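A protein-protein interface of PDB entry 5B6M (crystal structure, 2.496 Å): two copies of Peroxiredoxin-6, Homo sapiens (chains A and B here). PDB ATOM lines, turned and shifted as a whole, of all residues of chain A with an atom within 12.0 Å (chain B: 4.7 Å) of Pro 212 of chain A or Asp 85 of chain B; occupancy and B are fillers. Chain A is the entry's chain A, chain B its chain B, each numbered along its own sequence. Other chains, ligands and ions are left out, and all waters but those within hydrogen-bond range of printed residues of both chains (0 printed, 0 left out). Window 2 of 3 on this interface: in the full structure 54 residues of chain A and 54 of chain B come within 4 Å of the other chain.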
ATOM      1  N   MET A 188     -13.717 -15.317  20.517  1.00  0.00           N
ATOM      2  CA  MET A 188     -13.073 -15.126  19.223  1.00  0.00           C
ATOM      3  C   MET A 188     -11.813 -14.276  19.409  1.00  0.00           C
ATOM      4  O   MET A 188     -11.817 -13.319  20.203  1.00  0.00           O
ATOM      5  CB  MET A 188     -14.013 -14.395  18.242  1.00  0.00           C
ATOM      6  CG  MET A 188     -15.409 -14.974  18.081  1.00  0.00           C
ATOM      7  SD  MET A 188     -15.451 -16.779  18.004  1.00  0.00           S
ATOM      8  CE  MET A 188     -14.915 -17.119  16.321  1.00  0.00           C
ATOM      9  N   PRO A 191      -9.677  -9.741  15.092  1.00  0.00           N
ATOM     10  CA  PRO A 191      -9.258  -9.954  13.697  1.00  0.00           C
ATOM     11  C   PRO A 191      -7.936  -9.278  13.370  1.00  0.00           C
ATOM     12  O   PRO A 191      -7.336  -9.561  12.329  1.00  0.00           O
ATOM     13  CB  PRO A 191     -10.367  -9.267  12.900  1.00  0.00           C
ATOM     14  CG  PRO A 191     -10.867  -8.199  13.828  1.00  0.00           C
ATOM     15  CD  PRO A 191     -10.841  -8.846  15.182  1.00  0.00           C
ATOM     16  N   THR A 208      -8.304 -21.964  14.037  1.00  0.00           N
ATOM     17  CA  THR A 208      -8.710 -21.213  12.880  1.00  0.00           C
ATOM     18  C   THR A 208      -9.598 -22.116  12.046  1.00  0.00           C
ATOM     19  O   THR A 208      -9.287 -23.287  11.866  1.00  0.00           O
ATOM     20  CB  THR A 208      -7.478 -20.796  12.084  1.00  0.00           C
ATOM     21  OG1 THR A 208      -6.549 -20.155  12.963  1.00  0.00           O
ATOM     22  CG2 THR A 208      -7.848 -19.832  10.965  1.00  0.00           C
ATOM     23  N   LYS A 209     -10.729 -21.581  11.588  1.00  0.00           N
ATOM     24  CA  LYS A 209     -11.607 -22.294  10.665  1.00  0.00           C
ATOM     25  C   LYS A 209     -11.369 -21.786   9.241  1.00  0.00           C
ATOM     26  O   LYS A 209     -11.490 -20.585   8.956  1.00  0.00           O
ATOM     27  CB  LYS A 209     -13.074 -22.179  11.091  1.00  0.00           C
ATOM     28  CG  LYS A 209     -14.086 -22.245   9.963  1.00  0.00           C
ATOM     29  CD  LYS A 209     -14.075 -23.543   9.191  1.00  0.00           C
ATOM     30  CE  LYS A 209     -15.038 -24.549   9.764  1.00  0.00           C
ATOM     31  NZ  LYS A 209     -14.511 -25.164  11.015  1.00  0.00           N
ATOM     32  N   GLU A 210     -11.003 -22.716   8.365  1.00  0.00           N
ATOM     33  CA  GLU A 210     -10.647 -22.418   6.981  1.00  0.00           C
ATOM     34  C   GLU A 210     -11.893 -22.055   6.160  1.00  0.00           C
ATOM     35  O   GLU A 210     -12.908 -22.751   6.217  1.00  0.00           O
ATOM     36  CB  GLU A 210      -9.932 -23.633   6.382  1.00  0.00           C
ATOM     37  CG  GLU A 210      -8.478 -23.401   5.986  1.00  0.00           C
ATOM     38  CD  GLU A 210      -7.612 -22.827   7.101  1.00  0.00           C
ATOM     39  OE1 GLU A 210      -7.106 -21.692   6.910  1.00  0.00           O
ATOM     40  OE2 GLU A 210      -7.420 -23.513   8.146  1.00  0.00           O
ATOM     41  N   LEU A 211     -11.825 -20.967   5.403  1.00  0.00           N
ATOM     42  CA  LEU A 211     -13.020 -20.469   4.722  1.00  0.00           C
ATOM     43  C   LEU A 211     -12.822 -20.307   3.227  1.00  0.00           C
ATOM     44  O   LEU A 211     -11.697 -20.096   2.768  1.00  0.00           O
ATOM     45  CB  LEU A 211     -13.454 -19.136   5.335  1.00  0.00           C
ATOM     46  CG  LEU A 211     -13.862 -19.271   6.803  1.00  0.00           C
ATOM     47  CD1 LEU A 211     -13.846 -17.921   7.511  1.00  0.00           C
ATOM     48  CD2 LEU A 211     -15.217 -19.986   6.942  1.00  0.00           C
ATOM     49  N   PRO A 212     -13.922 -20.411   2.461  1.00  0.00           N
ATOM     50  CA  PRO A 212     -13.985 -20.172   1.014  1.00  0.00           C
ATOM     51  C   PRO A 212     -13.136 -18.987   0.516  1.00  0.00           C
ATOM     52  O   PRO A 212     -12.669 -18.994  -0.619  1.00  0.00           O
ATOM     53  CB  PRO A 212     -15.466 -19.882   0.795  1.00  0.00           C
ATOM     54  CG  PRO A 212     -16.135 -20.799   1.776  1.00  0.00           C
ATOM     55  CD  PRO A 212     -15.213 -20.891   2.981  1.00  0.00           C
ATOM     56  N   SER A 213     -12.958 -17.975   1.352  1.00  0.00           N
ATOM     57  CA  SER A 213     -12.132 -16.845   1.002  1.00  0.00           C
ATOM     58  C   SER A 213     -10.693 -17.114   1.450  1.00  0.00           C
ATOM     59  O   SER A 213      -9.793 -16.303   1.211  1.00  0.00           O
ATOM     60  CB  SER A 213     -12.670 -15.578   1.678  1.00  0.00           C
ATOM     61  OG  SER A 213     -12.521 -15.633   3.088  1.00  0.00           O
ATOM     62  N   GLY A 214     -10.478 -18.241   2.121  1.00  0.00           N
ATOM     63  CA  GLY A 214      -9.161 -18.566   2.635  1.00  0.00           C
ATOM     64  C   GLY A 214      -8.563 -17.517   3.555  1.00  0.00           C
ATOM     65  O   GLY A 214      -7.357 -17.522   3.775  1.00  0.00           O
ATOM     66  N   LYS A 215      -9.382 -16.610   4.082  1.00  0.00           N
ATOM     67  CA  LYS A 215      -8.885 -15.631   5.049  1.00  0.00           C
ATOM     68  C   LYS A 215      -8.856 -16.319   6.400  1.00  0.00           C
ATOM     69  O   LYS A 215      -9.565 -17.305   6.603  1.00  0.00           O
ATOM     70  CB  LYS A 215      -9.777 -14.373   5.110  1.00  0.00           C
ATOM     71  CG  LYS A 215     -10.085 -13.708   3.767  1.00  0.00           C
ATOM     72  CD  LYS A 215     -10.598 -12.292   3.966  1.00  0.00           C
ATOM     73  CE  LYS A 215     -10.643 -11.518   2.656  1.00  0.00           C
ATOM     74  NZ  LYS A 215     -10.440 -10.058   2.854  1.00  0.00           N
ATOM     75  N   LYS A 216      -8.051 -15.809   7.322  1.00  0.00           N
ATOM     76  CA  LYS A 216      -7.862 -16.497   8.595  1.00  0.00           C
ATOM     77  C   LYS A 216      -8.413 -15.754   9.805  1.00  0.00           C
ATOM     78  O   LYS A 216      -7.794 -15.739  10.859  1.00  0.00           O
ATOM     79  CB  LYS A 216      -6.383 -16.836   8.792  1.00  0.00           C
ATOM     80  CG  LYS A 216      -5.871 -17.878   7.796  1.00  0.00           C
ATOM     81  CD  LYS A 216      -4.383 -18.209   7.998  1.00  0.00           C
ATOM     82  CE  LYS A 216      -3.870 -19.219   6.963  1.00  0.00           C
ATOM     83  NZ  LYS A 216      -4.692 -20.458   6.986  1.00  0.00           N
ATOM     84  N   TYR A 217      -9.596 -15.171   9.665  1.00  0.00           N
ATOM     85  CA  TYR A 217     -10.181 -14.366  10.735  1.00  0.00           C
ATOM     86  C   TYR A 217     -10.966 -15.164  11.768  1.00  0.00           C
ATOM     87  O   TYR A 217     -11.074 -14.773  12.936  1.00  0.00           O
ATOM     88  CB  TYR A 217     -11.090 -13.287  10.148  1.00  0.00           C
ATOM     89  CG  TYR A 217     -12.256 -13.785   9.299  1.00  0.00           C
ATOM     90  CD1 TYR A 217     -13.508 -14.042   9.870  1.00  0.00           C
ATOM     91  CD2 TYR A 217     -12.119 -13.954   7.926  1.00  0.00           C
ATOM     92  CE1 TYR A 217     -14.580 -14.473   9.099  1.00  0.00           C
ATOM     93  CE2 TYR A 217     -13.190 -14.382   7.144  1.00  0.00           C
ATOM     94  CZ  TYR A 217     -14.422 -14.629   7.736  1.00  0.00           C
ATOM     95  OH  TYR A 217     -15.478 -15.055   6.964  1.00  0.00           O
ATOM     96  N   LEU A 218     -11.526 -16.279  11.318  1.00  0.00           N
ATOM     97  CA  LEU A 218     -12.432 -17.058  12.136  1.00  0.00           C
ATOM     98  C   LEU A 218     -11.636 -17.934  13.103  1.00  0.00           C
ATOM     99  O   LEU A 218     -11.350 -19.089  12.815  1.00  0.00           O
ATOM    100  CB  LEU A 218     -13.360 -17.885  11.242  1.00  0.00           C
ATOM    101  CG  LEU A 218     -14.609 -18.460  11.913  1.00  0.00           C
ATOM    102  CD1 LEU A 218     -15.336 -17.406  12.736  1.00  0.00           C
ATOM    103  CD2 LEU A 218     -15.527 -19.033  10.842  1.00  0.00           C
ATOM    104  N   ARG A 219     -11.285 -17.360  14.249  1.00  0.00           N
ATOM    105  CA  ARG A 219     -10.362 -17.977  15.186  1.00  0.00           C
ATOM    106  C   ARG A 219     -10.930 -17.998  16.611  1.00  0.00           C
ATOM    107  O   ARG A 219     -11.153 -16.944  17.221  1.00  0.00           O
ATOM    108  CB  ARG A 219      -9.036 -17.215  15.183  1.00  0.00           C
ATOM    109  CG  ARG A 219      -8.328 -17.174  13.846  1.00  0.00           C
ATOM    110  CD  ARG A 219      -6.941 -16.573  13.993  1.00  0.00           C
ATOM    111  NE  ARG A 219      -6.995 -15.148  14.288  1.00  0.00           N
ATOM    112  CZ  ARG A 219      -5.933 -14.390  14.543  1.00  0.00           C
ATOM    113  NH1 ARG A 219      -4.723 -14.915  14.545  1.00  0.00           N
ATOM    114  NH2 ARG A 219      -6.082 -13.099  14.793  1.00  0.00           N
ATOM    115  N   TYR A 220     -11.154 -19.202  17.134  1.00  0.00           N
ATOM    116  CA  TYR A 220     -11.606 -19.379  18.508  1.00  0.00           C
ATOM    117  C   TYR A 220     -10.423 -19.626  19.437  1.00  0.00           C
ATOM    118  O   TYR A 220      -9.362 -20.083  19.009  1.00  0.00           O
ATOM    119  CB  TYR A 220     -12.538 -20.573  18.615  1.00  0.00           C
ATOM    120  CG  TYR A 220     -13.591 -20.653  17.552  1.00  0.00           C
ATOM    121  CD1 TYR A 220     -13.275 -21.064  16.268  1.00  0.00           C
ATOM    122  CD2 TYR A 220     -14.912 -20.358  17.835  1.00  0.00           C
ATOM    123  CE1 TYR A 220     -14.247 -21.161  15.282  1.00  0.00           C
ATOM    124  CE2 TYR A 220     -15.885 -20.445  16.867  1.00  0.00           C
ATOM    125  CZ  TYR A 220     -15.552 -20.851  15.586  1.00  0.00           C
ATOM    126  OH  TYR A 220     -16.515 -20.949  14.597  1.00  0.00           O
ATOM    127  N   PHE B  43     -15.911 -10.190   7.187  1.00  0.00           N
ATOM    128  CA  PHE B  43     -14.676 -10.960   7.334  1.00  0.00           C
ATOM    129  C   PHE B  43     -14.097 -10.822   8.730  1.00  0.00           C
ATOM    130  O   PHE B  43     -12.885 -10.844   8.915  1.00  0.00           O
ATOM    131  CB  PHE B  43     -13.624 -10.570   6.283  1.00  0.00           C
ATOM    132  CG  PHE B  43     -14.113 -10.669   4.869  1.00  0.00           C
ATOM    133  CD1 PHE B  43     -14.432 -11.912   4.312  1.00  0.00           C
ATOM    134  CD2 PHE B  43     -14.251  -9.515   4.091  1.00  0.00           C
ATOM    135  CE1 PHE B  43     -14.886 -12.014   3.010  1.00  0.00           C
ATOM    136  CE2 PHE B  43     -14.715  -9.595   2.782  1.00  0.00           C
ATOM    137  CZ  PHE B  43     -15.033 -10.854   2.237  1.00  0.00           C
ATOM    138  N   ALA B  81     -19.148 -11.674  -1.202  1.00  0.00           N
ATOM    139  CA  ALA B  81     -18.049 -12.610  -0.996  1.00  0.00           C
ATOM    140  C   ALA B  81     -18.202 -13.300   0.371  1.00  0.00           C
ATOM    141  O   ALA B  81     -18.255 -14.533   0.458  1.00  0.00           O
ATOM    142  CB  ALA B  81     -16.691 -11.890  -1.127  1.00  0.00           C
ATOM    143  N   TRP B  82     -18.309 -12.482   1.418  1.00  0.00           N
ATOM    144  CA  TRP B  82     -18.419 -12.935   2.805  1.00  0.00           C
ATOM    145  C   TRP B  82     -19.664 -13.802   3.089  1.00  0.00           C
ATOM    146  O   TRP B  82     -19.700 -14.534   4.068  1.00  0.00           O
ATOM    147  CB  TRP B  82     -18.357 -11.711   3.733  1.00  0.00           C
ATOM    148  CG  TRP B  82     -18.428 -11.973   5.205  1.00  0.00           C
ATOM    149  CD1 TRP B  82     -17.652 -12.827   5.932  1.00  0.00           C
ATOM    150  CD2 TRP B  82     -19.298 -11.329   6.139  1.00  0.00           C
ATOM    151  NE1 TRP B  82     -18.007 -12.782   7.256  1.00  0.00           N
ATOM    152  CE2 TRP B  82     -19.013 -11.866   7.416  1.00  0.00           C
ATOM    153  CE3 TRP B  82     -20.313 -10.367   6.020  1.00  0.00           C
ATOM    154  CZ2 TRP B  82     -19.701 -11.468   8.570  1.00  0.00           C
ATOM    155  CZ3 TRP B  82     -20.999  -9.973   7.164  1.00  0.00           C
ATOM    156  CH2 TRP B  82     -20.692 -10.526   8.421  1.00  0.00           C
ATOM    157  N   SER B  83     -20.667 -13.750   2.224  1.00  0.00           N
ATOM    158  CA  SER B  83     -21.829 -14.617   2.394  1.00  0.00           C
ATOM    159  C   SER B  83     -21.436 -16.052   2.126  1.00  0.00           C
ATOM    160  O   SER B  83     -22.027 -16.977   2.690  1.00  0.00           O
ATOM    161  CB  SER B  83     -22.972 -14.219   1.458  1.00  0.00           C
ATOM    162  OG  SER B  83     -23.192 -12.828   1.499  1.00  0.00           O
ATOM    163  N   LYS B  84     -20.447 -16.234   1.252  1.00  0.00           N
ATOM    164  CA  LYS B  84     -19.914 -17.569   1.004  1.00  0.00           C
ATOM    165  C   LYS B  84     -19.293 -18.120   2.296  1.00  0.00           C
ATOM    166  O   LYS B  84     -19.470 -19.295   2.636  1.00  0.00           O
ATOM    167  CB  LYS B  84     -18.881 -17.561  -0.123  1.00  0.00           C
ATOM    168  CG  LYS B  84     -19.352 -16.994  -1.467  1.00  0.00           C
ATOM    169  CD  LYS B  84     -18.139 -16.821  -2.401  1.00  0.00           C
ATOM    170  CE  LYS B  84     -18.511 -16.548  -3.860  1.00  0.00           C
ATOM    171  NZ  LYS B  84     -17.338 -15.982  -4.621  1.00  0.00           N
ATOM    172  N   ASP B  85     -18.573 -17.273   3.027  1.00  0.00           N
ATOM    173  CA  ASP B  85     -18.071 -17.689   4.335  1.00  0.00           C
ATOM    174  C   ASP B  85     -19.195 -17.934   5.355  1.00  0.00           C
ATOM    175  O   ASP B  85     -19.186 -18.960   6.027  1.00  0.00           O
ATOM    176  CB  ASP B  85     -17.063 -16.688   4.889  1.00  0.00           C
ATOM    177  CG  ASP B  85     -15.810 -16.598   4.056  1.00  0.00           C
ATOM    178  OD1 ASP B  85     -15.679 -17.303   3.031  1.00  0.00           O
ATOM    179  OD2 ASP B  85     -14.941 -15.806   4.452  1.00  0.00           O
ATOM    180  N   ILE B  86     -20.140 -16.993   5.468  1.00  0.00           N
ATOM    181  CA  ILE B  86     -21.334 -17.178   6.300  1.00  0.00           C
ATOM    182  C   ILE B  86     -21.932 -18.551   6.013  1.00  0.00           C
ATOM    183  O   ILE B  86     -22.140 -19.362   6.920  1.00  0.00           O
ATOM    184  CB  ILE B  86     -22.498 -16.141   6.008  1.00  0.00           C
ATOM    185  CG1 ILE B  86     -22.050 -14.680   6.068  1.00  0.00           C
ATOM    186  CG2 ILE B  86     -23.673 -16.381   6.954  1.00  0.00           C
ATOM    187  CD1 ILE B  86     -21.356 -14.315   7.299  1.00  0.00           C
ATOM    188  N   ASN B  87     -22.231 -18.793   4.738  1.00  0.00           N
ATOM    189  CA  ASN B  87     -22.796 -20.079   4.335  1.00  0.00           C
ATOM    190  C   ASN B  87     -21.919 -21.302   4.670  1.00  0.00           C
ATOM    191  O   ASN B  87     -22.424 -22.310   5.150  1.00  0.00           O
ATOM    192  CB  ASN B  87     -23.246 -20.056   2.865  1.00  0.00           C
ATOM    193  CG  ASN B  87     -24.543 -19.270   2.676  1.00  0.00           C
ATOM    194  OD1 ASN B  87     -25.601 -19.649   3.205  1.00  0.00           O
ATOM    195  ND2 ASN B  87     -24.468 -18.167   1.924  1.00  0.00           N
ATOM    196  N   ALA B  88     -20.616 -21.191   4.424  1.00  0.00           N
ATOM    197  CA  ALA B  88     -19.675 -22.226   4.809  1.00  0.00           C
ATOM    198  C   ALA B  88     -19.788 -22.442   6.303  1.00  0.00           C
ATOM    199  O   ALA B  88     -20.118 -23.553   6.750  1.00  0.00           O
ATOM    200  CB  ALA B  88     -18.268 -21.840   4.446  1.00  0.00           C
ATOM    201  N   TYR B  89     -19.534 -21.387   7.075  1.00  0.00           N
ATOM    202  CA  TYR B  89     -19.685 -21.464   8.525  1.00  0.00           C
ATOM    203  C   TYR B  89     -20.961 -22.230   8.981  1.00  0.00           C
ATOM    204  O   TYR B  89     -20.938 -22.961   9.979  1.00  0.00           O
ATOM    205  CB  TYR B  89     -19.620 -20.060   9.142  1.00  0.00           C
ATOM    206  CG  TYR B  89     -19.987 -20.026  10.607  1.00  0.00           C
ATOM    207  CD1 TYR B  89     -19.014 -20.183  11.586  1.00  0.00           C
ATOM    208  CD2 TYR B  89     -21.309 -19.848  11.010  1.00  0.00           C
ATOM    209  CE1 TYR B  89     -19.339 -20.169  12.921  1.00  0.00           C
ATOM    210  CE2 TYR B  89     -21.644 -19.837  12.344  1.00  0.00           C
ATOM    211  CZ  TYR B  89     -20.653 -19.994  13.295  1.00  0.00           C
ATOM    212  OH  TYR B  89     -20.971 -19.976  14.620  1.00  0.00           O
ATOM    213  N   PRO B  94     -21.771 -22.807  -0.260  1.00  0.00           N
ATOM    214  CA  PRO B  94     -21.150 -21.482  -0.162  1.00  0.00           C
ATOM    215  C   PRO B  94     -21.455 -20.500  -1.298  1.00  0.00           C
ATOM    216  O   PRO B  94     -20.537 -19.830  -1.805  1.00  0.00           O
ATOM    217  CB  PRO B  94     -19.652 -21.804  -0.144  1.00  0.00           C
ATOM    218  CG  PRO B  94     -19.549 -23.095  -0.857  1.00  0.00           C
ATOM    219  CD  PRO B  94     -20.765 -23.864  -0.433  1.00  0.00           C
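Lys 209 of chain A touches none of the printed residues of chain B.
Pro 212 of chain A touches three residues of chain B.
Lys 216 of chain A touches none of the printed residues of chain B.
Of the printed residues of chain B, Leu 218 of chain A touches Tyr 89 (3.7 Å).
No residue of chain A comes within 4 Å of Ala 81 of chain B.
Of the printed residues of chain A, Trp 82 of chain B touches Tyr 217.
Lys 84 of chain B touches just one residue of chain A: Pro 212 (3.8 Å).
Asp 85 of chain B touches just these residues of chain A: Leu 211 (3.7 Å), Pro 212 (3.4 Å), Ser 213 (2.8 Å) and Tyr 217 (2.7 Å).
No residue of chain A comes within 4 Å of Ile 86 of chain B.
No residue of chain A comes within 4 Å of Asn 87 of chain B.
Of chain A, only Pro 212 (3.5 Å) comes within 4 Å of Ala 88 of chain B.
The nearest printed residue of chain A that does not touch Asp 85 of chain B is Lys 215 of chain A (5.3 Å).
The nearest printed residue of chain A that does not touch Trp 82 of chain B is Ser 213 of chain A (6.4 Å).
Among the printed residues, pairs that only touch across the chains: Leu 211 of chain A with Asp 85 of chain B (3.7 Å), Pro 212 of chain A with Lys 84 of chain B (3.8 Å), Pro 212 of chain A with Asp 85 of chain B (3.4 Å), Pro 212 of chain A with Ala 88 of chain B (3.5 Å), Lys 215 of chain A with Phe 43 of chain B (3.9 Å), Tyr 217 of chain A with Phe 43 of chain B (3.0 Å), Leu 218 of chain A with Tyr 89 of chain B (3.7 Å) and Tyr 220 of chain A with Tyr 89 of chain B (3.4 Å).
Of the 11 printed residues of chain B, 6 touch a printed residue of chain A.
Hydrophobic or aromatic side chains of chain B that line the printed part of chain A: Phe 43, Trp 82, Ala 88 and Tyr 89.
Printed residues of chain A that touch a printed residue of chain B: Leu 211, Pro 212, Ser 213, Lys 215, Tyr 217, Leu 218 and Tyr 220.
Among the printed residues, 11 pairs touch across the chains.
Among the printed residues, no Asp or Glu carboxylate lies within 4 Å of a Lys or Arg side-chain nitrogen of the other chain.
No position is printed for both chains.
Of the 11 pairs that touch across the chains among the printed residues, none has its exchanged pair printed and touching as well.
OG of Ser 213 of chain A sits at hydrogen-bond distance from OD2 of Asp 85 of chain B (2.8 Å).
The side-chain hydroxyl (OH) of Tyr 217 of chain A sits close to the indole nitrogen (NE1) of Trp 82 of chain B (3.4 Å).
The side-chain hydroxyl (OH) of Tyr 217 of chain A lies within hydrogen-bond range of the side-chain carboxylate (OD2) of Asp 85 of chain B (2.7 Å).
N of Lys 209 of chain A is in hydrogen-bond range of O of Leu 218 of chain A (2.8 Å).
The backbone NH (N) of Lys 215 of chain A lies close to the side-chain hydroxyl (OG) of Ser 213 of chain A (3.4 Å).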
